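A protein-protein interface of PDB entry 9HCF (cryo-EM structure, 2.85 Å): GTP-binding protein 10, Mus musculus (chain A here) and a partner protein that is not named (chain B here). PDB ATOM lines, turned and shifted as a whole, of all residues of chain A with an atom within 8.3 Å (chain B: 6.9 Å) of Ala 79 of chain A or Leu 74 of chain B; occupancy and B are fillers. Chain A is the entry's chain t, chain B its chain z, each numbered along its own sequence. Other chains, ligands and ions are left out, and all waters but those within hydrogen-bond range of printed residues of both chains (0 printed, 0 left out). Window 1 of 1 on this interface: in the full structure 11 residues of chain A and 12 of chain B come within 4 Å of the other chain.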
ATOM      1  N   TYR A  32       0.945  26.065   5.523  1.00  0.00           N
ATOM      2  CA  TYR A  32       2.193  26.090   6.275  1.00  0.00           C
ATOM      3  C   TYR A  32       3.063  24.923   5.839  1.00  0.00           C
ATOM      4  O   TYR A  32       2.685  23.768   6.087  1.00  0.00           O
ATOM      5  CB  TYR A  32       1.906  26.010   7.770  1.00  0.00           C
ATOM      6  CG  TYR A  32       3.137  25.902   8.639  1.00  0.00           C
ATOM      7  CD1 TYR A  32       3.845  27.034   9.013  1.00  0.00           C
ATOM      8  CD2 TYR A  32       3.586  24.669   9.090  1.00  0.00           C
ATOM      9  CE1 TYR A  32       4.970  26.941   9.811  1.00  0.00           C
ATOM     10  CE2 TYR A  32       4.708  24.566   9.887  1.00  0.00           C
ATOM     11  CZ  TYR A  32       5.396  25.705  10.245  1.00  0.00           C
ATOM     12  OH  TYR A  32       6.515  25.611  11.040  1.00  0.00           O
ATOM     13  N   PRO A  33       4.224  25.145   5.226  1.00  0.00           N
ATOM     14  CA  PRO A  33       4.953  24.030   4.606  1.00  0.00           C
ATOM     15  C   PRO A  33       5.404  23.001   5.632  1.00  0.00           C
ATOM     16  O   PRO A  33       5.403  23.230   6.843  1.00  0.00           O
ATOM     17  CB  PRO A  33       6.154  24.704   3.930  1.00  0.00           C
ATOM     18  CG  PRO A  33       5.860  26.171   3.945  1.00  0.00           C
ATOM     19  CD  PRO A  33       4.972  26.408   5.115  1.00  0.00           C
ATOM     20  N   ARG A  34       5.794  21.837   5.112  1.00  0.00           N
ATOM     21  CA  ARG A  34       6.256  20.712   5.924  1.00  0.00           C
ATOM     22  C   ARG A  34       5.150  20.210   6.857  1.00  0.00           C
ATOM     23  O   ARG A  34       5.264  20.247   8.084  1.00  0.00           O
ATOM     24  CB  ARG A  34       7.513  21.094   6.711  1.00  0.00           C
ATOM     25  CG  ARG A  34       8.624  21.663   5.844  1.00  0.00           C
ATOM     26  CD  ARG A  34       9.898  21.892   6.639  1.00  0.00           C
ATOM     27  NE  ARG A  34      10.493  23.193   6.353  1.00  0.00           N
ATOM     28  CZ  ARG A  34      11.498  23.725   7.036  1.00  0.00           C
ATOM     29  NH1 ARG A  34      12.059  23.089   8.051  1.00  0.00           N
ATOM     30  NH2 ARG A  34      11.952  24.926   6.690  1.00  0.00           N
ATOM     31  N   LEU A  35       4.062  19.747   6.242  1.00  0.00           N
ATOM     32  CA  LEU A  35       2.960  19.031   6.888  1.00  0.00           C
ATOM     33  C   LEU A  35       1.999  19.972   7.605  1.00  0.00           C
ATOM     34  O   LEU A  35       1.127  19.500   8.346  1.00  0.00           O
ATOM     35  CB  LEU A  35       3.475  17.973   7.872  1.00  0.00           C
ATOM     36  CG  LEU A  35       2.473  16.990   8.492  1.00  0.00           C
ATOM     37  CD1 LEU A  35       1.675  16.253   7.426  1.00  0.00           C
ATOM     38  CD2 LEU A  35       3.200  15.998   9.388  1.00  0.00           C
ATOM     39  N   GLY A  36       2.113  21.284   7.403  1.00  0.00           N
ATOM     40  CA  GLY A  36       1.172  22.193   8.039  1.00  0.00           C
ATOM     41  C   GLY A  36      -0.258  21.936   7.606  1.00  0.00           C
ATOM     42  O   GLY A  36      -1.192  22.080   8.398  1.00  0.00           O
ATOM     43  N   GLY A  37      -0.449  21.561   6.349  1.00  0.00           N
ATOM     44  CA  GLY A  37      -1.747  21.149   5.866  1.00  0.00           C
ATOM     45  C   GLY A  37      -2.453  22.203   5.039  1.00  0.00           C
ATOM     46  O   GLY A  37      -1.856  23.133   4.492  1.00  0.00           O
ATOM     47  N   GLU A  38      -3.769  22.039   4.956  1.00  0.00           N
ATOM     48  CA  GLU A  38      -4.600  22.832   4.069  1.00  0.00           C
ATOM     49  C   GLU A  38      -4.835  24.227   4.638  1.00  0.00           C
ATOM     50  O   GLU A  38      -4.674  24.480   5.836  1.00  0.00           O
ATOM     51  CB  GLU A  38      -5.944  22.140   3.842  1.00  0.00           C
ATOM     52  CG  GLU A  38      -5.833  20.760   3.221  1.00  0.00           C
ATOM     53  CD  GLU A  38      -7.187  20.124   2.972  1.00  0.00           C
ATOM     54  OE1 GLU A  38      -8.200  20.677   3.450  1.00  0.00           O
ATOM     55  OE2 GLU A  38      -7.238  19.073   2.300  1.00  0.00           O
ATOM     56  N   GLY A  39      -5.216  25.140   3.751  1.00  0.00           N
ATOM     57  CA  GLY A  39      -5.693  26.450   4.139  1.00  0.00           C
ATOM     58  C   GLY A  39      -7.208  26.505   4.076  1.00  0.00           C
ATOM     59  O   GLY A  39      -7.839  25.785   3.306  1.00  0.00           O
ATOM     60  N   ASN A  74      -4.792  31.340   7.397  1.00  0.00           N
ATOM     61  CA  ASN A  74      -3.646  30.568   6.941  1.00  0.00           C
ATOM     62  C   ASN A  74      -3.311  29.475   7.947  1.00  0.00           C
ATOM     63  O   ASN A  74      -3.467  29.644   9.159  1.00  0.00           O
ATOM     64  CB  ASN A  74      -2.432  31.475   6.741  1.00  0.00           C
ATOM     65  CG  ASN A  74      -2.782  32.781   6.060  1.00  0.00           C
ATOM     66  OD1 ASN A  74      -3.274  32.795   4.932  1.00  0.00           O
ATOM     67  ND2 ASN A  74      -2.530  33.891   6.744  1.00  0.00           N
ATOM     68  N   SER A  75      -2.848  28.340   7.431  1.00  0.00           N
ATOM     69  CA  SER A  75      -2.465  27.238   8.303  1.00  0.00           C
ATOM     70  C   SER A  75      -1.339  27.677   9.227  1.00  0.00           C
ATOM     71  O   SER A  75      -0.396  28.355   8.808  1.00  0.00           O
ATOM     72  CB  SER A  75      -2.034  26.030   7.474  1.00  0.00           C
ATOM     73  OG  SER A  75      -1.817  24.898   8.298  1.00  0.00           O
ATOM     74  N   ARG A  76      -1.437  27.285  10.491  1.00  0.00           N
ATOM     75  CA  ARG A  76      -0.512  27.712  11.530  1.00  0.00           C
ATOM     76  C   ARG A  76       0.345  26.542  11.988  1.00  0.00           C
ATOM     77  O   ARG A  76       0.085  25.379  11.666  1.00  0.00           O
ATOM     78  CB  ARG A  76      -1.267  28.303  12.726  1.00  0.00           C
ATOM     79  CG  ARG A  76      -2.213  29.439  12.379  1.00  0.00           C
ATOM     80  CD  ARG A  76      -3.040  29.846  13.588  1.00  0.00           C
ATOM     81  NE  ARG A  76      -4.053  30.839  13.253  1.00  0.00           N
ATOM     82  CZ  ARG A  76      -5.002  31.253  14.082  1.00  0.00           C
ATOM     83  NH1 ARG A  76      -5.105  30.773  15.311  1.00  0.00           N
ATOM     84  NH2 ARG A  76      -5.871  32.170  13.668  1.00  0.00           N
ATOM     85  N   VAL A  77       1.389  26.871  12.752  1.00  0.00           N
ATOM     86  CA  VAL A  77       2.232  25.835  13.326  1.00  0.00           C
ATOM     87  C   VAL A  77       1.353  24.877  14.121  1.00  0.00           C
ATOM     88  O   VAL A  77       0.285  25.248  14.625  1.00  0.00           O
ATOM     89  CB  VAL A  77       3.335  26.440  14.211  1.00  0.00           C
ATOM     90  CG1 VAL A  77       4.217  25.344  14.791  1.00  0.00           C
ATOM     91  CG2 VAL A  77       4.170  27.436  13.419  1.00  0.00           C
ATOM     92  N   SER A  78       1.802  23.630  14.223  1.00  0.00           N
ATOM     93  CA  SER A  78       1.065  22.514  14.810  1.00  0.00           C
ATOM     94  C   SER A  78       0.058  21.953  13.816  1.00  0.00           C
ATOM     95  O   SER A  78      -0.807  21.152  14.203  1.00  0.00           O
ATOM     96  CB  SER A  78       0.340  22.892  16.106  1.00  0.00           C
ATOM     97  OG  SER A  78       1.212  23.552  17.006  1.00  0.00           O
ATOM     98  N   ALA A  79       0.138  22.352  12.546  1.00  0.00           N
ATOM     99  CA  ALA A  79      -0.728  21.825  11.492  1.00  0.00           C
ATOM    100  C   ALA A  79      -2.198  22.132  11.763  1.00  0.00           C
ATOM    101  O   ALA A  79      -3.083  21.329  11.463  1.00  0.00           O
ATOM    102  CB  ALA A  79      -0.517  20.321  11.312  1.00  0.00           C
ATOM    103  N   LEU A  80      -2.467  23.304  12.333  1.00  0.00           N
ATOM    104  CA  LEU A  80      -3.844  23.753  12.467  1.00  0.00           C
ATOM    105  C   LEU A  80      -4.463  23.925  11.087  1.00  0.00           C
ATOM    106  O   LEU A  80      -3.870  24.548  10.203  1.00  0.00           O
ATOM    107  CB  LEU A  80      -3.908  25.072  13.239  1.00  0.00           C
ATOM    108  CG  LEU A  80      -4.055  24.970  14.759  1.00  0.00           C
ATOM    109  CD1 LEU A  80      -2.817  24.357  15.380  1.00  0.00           C
ATOM    110  CD2 LEU A  80      -4.337  26.338  15.363  1.00  0.00           C
ATOM    111  N   GLN A  81      -5.653  23.368  10.899  1.00  0.00           N
ATOM    112  CA  GLN A  81      -6.360  23.571   9.648  1.00  0.00           C
ATOM    113  C   GLN A  81      -6.996  24.958   9.629  1.00  0.00           C
ATOM    114  O   GLN A  81      -7.184  25.599  10.666  1.00  0.00           O
ATOM    115  CB  GLN A  81      -7.424  22.493   9.440  1.00  0.00           C
ATOM    116  CG  GLN A  81      -8.033  22.495   8.045  1.00  0.00           C
ATOM    117  CD  GLN A  81      -8.848  21.251   7.757  1.00  0.00           C
ATOM    118  OE1 GLN A  81      -8.713  20.235   8.437  1.00  0.00           O
ATOM    119  NE2 GLN A  81      -9.702  21.326   6.743  1.00  0.00           N
ATOM    120  N   GLY A  82      -7.329  25.416   8.427  1.00  0.00           N
ATOM    121  CA  GLY A  82      -7.854  26.755   8.275  1.00  0.00           C
ATOM    122  C   GLY A  82      -9.202  26.930   8.946  1.00  0.00           C
ATOM    123  O   GLY A  82      -9.938  25.978   9.209  1.00  0.00           O
ATOM    124  N   LYS A 126      -3.851  24.927  -0.396  1.00  0.00           N
ATOM    125  CA  LYS A 126      -3.260  23.679   0.071  1.00  0.00           C
ATOM    126  C   LYS A 126      -1.853  23.579  -0.492  1.00  0.00           C
ATOM    127  O   LYS A 126      -1.663  23.636  -1.710  1.00  0.00           O
ATOM    128  CB  LYS A 126      -4.107  22.476  -0.354  1.00  0.00           C
ATOM    129  CG  LYS A 126      -5.546  22.537   0.135  1.00  0.00           C
ATOM    130  CD  LYS A 126      -6.300  21.247  -0.149  1.00  0.00           C
ATOM    131  CE  LYS A 126      -6.545  21.050  -1.633  1.00  0.00           C
ATOM    132  NZ  LYS A 126      -7.300  19.796  -1.902  1.00  0.00           N
ATOM    133  N   LEU A 127      -0.868  23.439   0.395  1.00  0.00           N
ATOM    134  CA  LEU A 127       0.517  23.380  -0.054  1.00  0.00           C
ATOM    135  C   LEU A 127       0.840  22.041  -0.701  1.00  0.00           C
ATOM    136  O   LEU A 127       1.679  21.978  -1.606  1.00  0.00           O
ATOM    137  CB  LEU A 127       1.448  23.645   1.127  1.00  0.00           C
ATOM    138  CG  LEU A 127       1.382  22.608   2.249  1.00  0.00           C
ATOM    139  CD1 LEU A 127       2.388  21.474   2.041  1.00  0.00           C
ATOM    140  CD2 LEU A 127       1.579  23.282   3.584  1.00  0.00           C
ATOM    141  N   HIS A 128       0.189  20.966  -0.253  1.00  0.00           N
ATOM    142  CA  HIS A 128       0.462  19.651  -0.816  1.00  0.00           C
ATOM    143  C   HIS A 128      -0.011  19.551  -2.263  1.00  0.00           C
ATOM    144  O   HIS A 128       0.641  18.904  -3.089  1.00  0.00           O
ATOM    145  CB  HIS A 128      -0.186  18.571   0.051  1.00  0.00           C
ATOM    146  CG  HIS A 128      -1.679  18.650   0.108  1.00  0.00           C
ATOM    147  ND1 HIS A 128      -2.496  18.025  -0.809  1.00  0.00           N
ATOM    148  CD2 HIS A 128      -2.503  19.276   0.982  1.00  0.00           C
ATOM    149  CE1 HIS A 128      -3.759  18.267  -0.505  1.00  0.00           C
ATOM    150  NE2 HIS A 128      -3.790  19.022   0.578  1.00  0.00           N
ATOM    151  N   GLN B  42      -7.060  20.245  18.103  1.00  0.00           N
ATOM    152  CA  GLN B  42      -6.434  20.990  17.017  1.00  0.00           C
ATOM    153  C   GLN B  42      -4.919  20.992  17.156  1.00  0.00           C
ATOM    154  O   GLN B  42      -4.195  20.805  16.171  1.00  0.00           O
ATOM    155  CB  GLN B  42      -6.968  22.422  16.989  1.00  0.00           C
ATOM    156  CG  GLN B  42      -8.424  22.524  16.589  1.00  0.00           C
ATOM    157  CD  GLN B  42      -8.669  22.032  15.186  1.00  0.00           C
ATOM    158  OE1 GLN B  42      -9.086  20.893  14.981  1.00  0.00           O
ATOM    159  NE2 GLN B  42      -8.420  22.891  14.205  1.00  0.00           N
ATOM    160  N   SER B  43      -4.419  21.201  18.374  1.00  0.00           N
ATOM    161  CA  SER B  43      -2.979  21.233  18.592  1.00  0.00           C
ATOM    162  C   SER B  43      -2.327  19.872  18.380  1.00  0.00           C
ATOM    163  O   SER B  43      -1.111  19.808  18.178  1.00  0.00           O
ATOM    164  CB  SER B  43      -2.678  21.740  20.003  1.00  0.00           C
ATOM    165  OG  SER B  43      -1.282  21.828  20.227  1.00  0.00           O
ATOM    166  N   SER B  44      -3.101  18.789  18.418  1.00  0.00           N
ATOM    167  CA  SER B  44      -2.563  17.441  18.299  1.00  0.00           C
ATOM    168  C   SER B  44      -2.508  16.944  16.860  1.00  0.00           C
ATOM    169  O   SER B  44      -2.136  15.788  16.636  1.00  0.00           O
ATOM    170  CB  SER B  44      -3.393  16.470  19.142  1.00  0.00           C
ATOM    171  OG  SER B  44      -3.288  16.775  20.522  1.00  0.00           O
ATOM    172  N   LEU B  45      -2.871  17.781  15.885  1.00  0.00           N
ATOM    173  CA  LEU B  45      -2.793  17.368  14.488  1.00  0.00           C
ATOM    174  C   LEU B  45      -1.368  17.010  14.091  1.00  0.00           C
ATOM    175  O   LEU B  45      -1.161  16.199  13.181  1.00  0.00           O
ATOM    176  CB  LEU B  45      -3.324  18.478  13.583  1.00  0.00           C
ATOM    177  CG  LEU B  45      -4.827  18.461  13.310  1.00  0.00           C
ATOM    178  CD1 LEU B  45      -5.168  17.356  12.325  1.00  0.00           C
ATOM    179  CD2 LEU B  45      -5.603  18.292  14.604  1.00  0.00           C
ATOM    180  N   LYS B  46      -0.380  17.625  14.744  1.00  0.00           N
ATOM    181  CA  LYS B  46       1.025  17.334  14.477  1.00  0.00           C
ATOM    182  C   LYS B  46       1.291  15.848  14.274  1.00  0.00           C
ATOM    183  O   LYS B  46       1.945  15.447  13.307  1.00  0.00           O
ATOM    184  CB  LYS B  46       1.875  17.857  15.636  1.00  0.00           C
ATOM    185  CG  LYS B  46       2.093  19.354  15.612  1.00  0.00           C
ATOM    186  CD  LYS B  46       2.970  19.844  16.762  1.00  0.00           C
ATOM    187  CE  LYS B  46       2.359  19.559  18.129  1.00  0.00           C
ATOM    188  NZ  LYS B  46       1.135  20.370  18.370  1.00  0.00           N
ATOM    189  N   SER B  47       0.784  15.014  15.183  1.00  0.00           N
ATOM    190  CA  SER B  47       1.255  13.643  15.335  1.00  0.00           C
ATOM    191  C   SER B  47       0.151  12.618  15.099  1.00  0.00           C
ATOM    192  O   SER B  47       0.104  11.589  15.775  1.00  0.00           O
ATOM    193  CB  SER B  47       1.868  13.449  16.718  1.00  0.00           C
ATOM    194  OG  SER B  47       0.880  13.541  17.729  1.00  0.00           O
ATOM    195  N   VAL B  51      -7.584   9.922  11.283  1.00  0.00           N
ATOM    196  CA  VAL B  51      -8.616  10.283  12.247  1.00  0.00           C
ATOM    197  C   VAL B  51      -9.798   9.344  12.056  1.00  0.00           C
ATOM    198  O   VAL B  51     -10.253   9.135  10.926  1.00  0.00           O
ATOM    199  CB  VAL B  51      -9.053  11.750  12.092  1.00  0.00           C
ATOM    200  CG1 VAL B  51      -9.883  12.182  13.290  1.00  0.00           C
ATOM    201  CG2 VAL B  51      -7.842  12.652  11.924  1.00  0.00           C
ATOM    202  N   PHE B  68     -15.733  18.155  12.709  1.00  0.00           N
ATOM    203  CA  PHE B  68     -14.718  17.117  12.561  1.00  0.00           C
ATOM    204  C   PHE B  68     -14.211  17.046  11.125  1.00  0.00           C
ATOM    205  O   PHE B  68     -13.002  16.968  10.886  1.00  0.00           O
ATOM    206  CB  PHE B  68     -15.281  15.766  13.004  1.00  0.00           C
ATOM    207  CG  PHE B  68     -15.541  15.667  14.484  1.00  0.00           C
ATOM    208  CD1 PHE B  68     -14.741  16.334  15.398  1.00  0.00           C
ATOM    209  CD2 PHE B  68     -16.588  14.898  14.960  1.00  0.00           C
ATOM    210  CE1 PHE B  68     -14.984  16.238  16.753  1.00  0.00           C
ATOM    211  CE2 PHE B  68     -16.833  14.799  16.315  1.00  0.00           C
ATOM    212  CZ  PHE B  68     -16.031  15.471  17.211  1.00  0.00           C
ATOM    213  N   GLN B  69     -15.120  17.074  10.150  1.00  0.00           N
ATOM    214  CA  GLN B  69     -14.677  17.143   8.761  1.00  0.00           C
ATOM    215  C   GLN B  69     -14.006  18.480   8.475  1.00  0.00           C
ATOM    216  O   GLN B  69     -13.038  18.546   7.710  1.00  0.00           O
ATOM    217  CB  GLN B  69     -15.854  16.917   7.812  1.00  0.00           C
ATOM    218  CG  GLN B  69     -15.515  17.176   6.351  1.00  0.00           C
ATOM    219  CD  GLN B  69     -16.574  16.653   5.399  1.00  0.00           C
ATOM    220  OE1 GLN B  69     -17.202  15.626   5.653  1.00  0.00           O
ATOM    221  NE2 GLN B  69     -16.773  17.360   4.293  1.00  0.00           N
ATOM    222  N   GLU B  70     -14.513  19.556   9.078  1.00  0.00           N
ATOM    223  CA  GLU B  70     -13.970  20.885   8.825  1.00  0.00           C
ATOM    224  C   GLU B  70     -12.603  21.056   9.475  1.00  0.00           C
ATOM    225  O   GLU B  70     -11.605  21.321   8.796  1.00  0.00           O
ATOM    226  CB  GLU B  70     -14.948  21.944   9.337  1.00  0.00           C
ATOM    227  CG  GLU B  70     -14.770  23.318   8.720  1.00  0.00           C
ATOM    228  CD  GLU B  70     -15.904  24.261   9.074  1.00  0.00           C
ATOM    229  OE1 GLU B  70     -16.970  23.775   9.509  1.00  0.00           O
ATOM    230  OE2 GLU B  70     -15.732  25.487   8.918  1.00  0.00           O
ATOM    231  N   LEU B  71     -12.537  20.908  10.800  1.00  0.00           N
ATOM    232  CA  LEU B  71     -11.283  21.134  11.511  1.00  0.00           C
ATOM    233  C   LEU B  71     -10.284  20.012  11.252  1.00  0.00           C
ATOM    234  O   LEU B  71      -9.104  20.268  10.988  1.00  0.00           O
ATOM    235  CB  LEU B  71     -11.549  21.273  13.009  1.00  0.00           C
ATOM    236  CG  LEU B  71     -12.461  22.412  13.464  1.00  0.00           C
ATOM    237  CD1 LEU B  71     -12.610  22.386  14.975  1.00  0.00           C
ATOM    238  CD2 LEU B  71     -11.921  23.756  13.009  1.00  0.00           C
ATOM    239  N   LEU B  72     -10.737  18.760  11.325  1.00  0.00           N
ATOM    240  CA  LEU B  72      -9.863  17.603  11.188  1.00  0.00           C
ATOM    241  C   LEU B  72      -9.855  17.050   9.768  1.00  0.00           C
ATOM    242  O   LEU B  72      -9.421  15.913   9.552  1.00  0.00           O
ATOM    243  CB  LEU B  72     -10.277  16.509  12.179  1.00  0.00           C
ATOM    244  CG  LEU B  72      -9.775  16.633  13.620  1.00  0.00           C
ATOM    245  CD1 LEU B  72      -8.262  16.554  13.670  1.00  0.00           C
ATOM    246  CD2 LEU B  72     -10.265  17.920  14.262  1.00  0.00           C
ATOM    247  N   GLY B  73     -10.320  17.833   8.792  1.00  0.00           N
ATOM    248  CA  GLY B  73     -10.320  17.382   7.412  1.00  0.00           C
ATOM    249  C   GLY B  73      -8.938  17.253   6.810  1.00  0.00           C
ATOM    250  O   GLY B  73      -8.784  16.600   5.772  1.00  0.00           O
ATOM    251  N   LEU B  74      -7.929  17.863   7.435  1.00  0.00           N
ATOM    252  CA  LEU B  74      -6.580  17.826   6.882  1.00  0.00           C
ATOM    253  C   LEU B  74      -6.086  16.391   6.737  1.00  0.00           C
ATOM    254  O   LEU B  74      -5.556  16.006   5.690  1.00  0.00           O
ATOM    255  CB  LEU B  74      -5.638  18.637   7.772  1.00  0.00           C
ATOM    256  CG  LEU B  74      -4.136  18.403   7.599  1.00  0.00           C
ATOM    257  CD1 LEU B  74      -3.712  18.599   6.151  1.00  0.00           C
ATOM    258  CD2 LEU B  74      -3.356  19.324   8.523  1.00  0.00           C
ATOM    259  N   LYS B  75      -6.261  15.585   7.776  1.00  0.00           N
ATOM    260  CA  LYS B  75      -5.831  14.197   7.751  1.00  0.00           C
ATOM    261  C   LYS B  75      -6.882  13.322   7.085  1.00  0.00           C
ATOM    262  O   LYS B  75      -8.058  13.691   7.005  1.00  0.00           O
ATOM    263  CB  LYS B  75      -5.573  13.701   9.171  1.00  0.00           C
ATOM    264  CG  LYS B  75      -4.112  13.729   9.587  1.00  0.00           C
ATOM    265  CD  LYS B  75      -3.609  15.147   9.764  1.00  0.00           C
ATOM    266  CE  LYS B  75      -2.280  15.175  10.498  1.00  0.00           C
ATOM    267  NZ  LYS B  75      -1.640  16.517  10.456  1.00  0.00           N
ATOM    268  N   PRO B  76      -6.492  12.148   6.595  1.00  0.00           N
ATOM    269  CA  PRO B  76      -7.485  11.227   6.037  1.00  0.00           C
ATOM    270  C   PRO B  76      -8.410  10.700   7.122  1.00  0.00           C
ATOM    271  O   PRO B  76      -8.057  10.646   8.302  1.00  0.00           O
ATOM    272  CB  PRO B  76      -6.631  10.111   5.429  1.00  0.00           C
ATOM    273  CG  PRO B  76      -5.373  10.130   6.219  1.00  0.00           C
ATOM    274  CD  PRO B  76      -5.137  11.570   6.588  1.00  0.00           C
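Among the printed residues, merely in contact across the chains: Gly 36 of chain A with Leu 74 of chain B (3.5 Å), Gly 37 of chain A with Leu 74 of chain B (3.2 Å), Glu 38 of chain A with Leu 74 of chain B (3.6 Å), Ser 78 of chain A with Gln 42 of chain B (3.9 Å), Ser 78 of chain A with Ser 43 of chain B (3.99 Å), Ser 78 of chain A with Leu 45 of chain B (3.7 Å), Ala 79 of chain A with Leu 45 of chain B (3.6 Å), Ala 79 of chain A with Leu 74 of chain B (3.6 Å), Leu 80 of chain A with Gln 42 of chain B (3.9 Å) and Gln 81 of chain A with Leu 72 of chain B (3.6 Å).
Leu 74 of chain B touches just these residues of chain A: Gly 36, Gly 37, Glu 38, Ala 79 and Gln 81. Of chain A, only Gln 81 comes within 4 Å of Gly 73 of chain B. Of the printed residues of chain B, Gly 36 of chain A touches Leu 74 (3.5 Å). Printed residues of chain B within 4 Å of Gln 81 of chain A: Glu 70, Leu 71, Leu 72, Gly 73 and Leu 74. Of the printed residues of chain B, Ser 78 of chain A touches Gln 42, Ser 43, Leu 45 and Lys 46. Ser 75 of chain A touches none of the printed residues of chain B. The nearest residue of chain A that does not touch Leu 74 of chain B is Leu 35 of chain A (4.5 Å).
Of the 16 printed residues of chain B, 9 touch a printed residue of chain A. Hydrophobic or aromatic side chains of chain B that line the printed part of chain A: Leu 45 and Leu 74. Of the 20 printed residues of chain A, 7 touch a printed residue of chain B. Among the printed residues, no Asp or Glu carboxylate lies within 4 Å of a Lys or Arg side-chain nitrogen of the other chain.
OG of Ser 43 of chain B sits at hydrogen-bond distance from NZ of Lys 46 of chain B (3.4 Å). The backbone carbonyl oxygen of Gly 36 of chain A lies within hydrogen-bond range of the side-chain hydroxyl of Ser 75 of chain A (2.9 Å). The side-chain hydroxyl (OG) of Ser 75 of chain A lies within hydrogen-bond range of the backbone carbonyl oxygen (O) of Leu 80 of chain A, 2.8 Å away. The backbone carbonyl oxygen (O) of Leu 45 of chain B lies within hydrogen-bond range of the side-chain amino group (NZ) of Lys 75 of chain B, 2.8 Å away.
The side-chain amino group (NZ) of Lys 46 of chain B is in hydrogen-bond range of the side-chain hydroxyl (OG) of Ser 78 of chain A. The backbone NH (N) of Gly 73 of chain B is in hydrogen-bond range of the side-chain amide oxygen (OE1) of Gln 81 of chain A (2.9 Å). The backbone NH of Leu 74 of chain B lies within hydrogen-bond range of the side-chain amide oxygen of Gln 81 of chain A, 2.7 Å away. O of Glu 70 of chain B is in hydrogen-bond range of NE2 of Gln 81 of chain A (2.8 Å). The backbone carbonyl oxygen of Leu 71 of chain B lies close to the side-chain amide oxygen of Gln 81 of chain A (2.6 Å).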
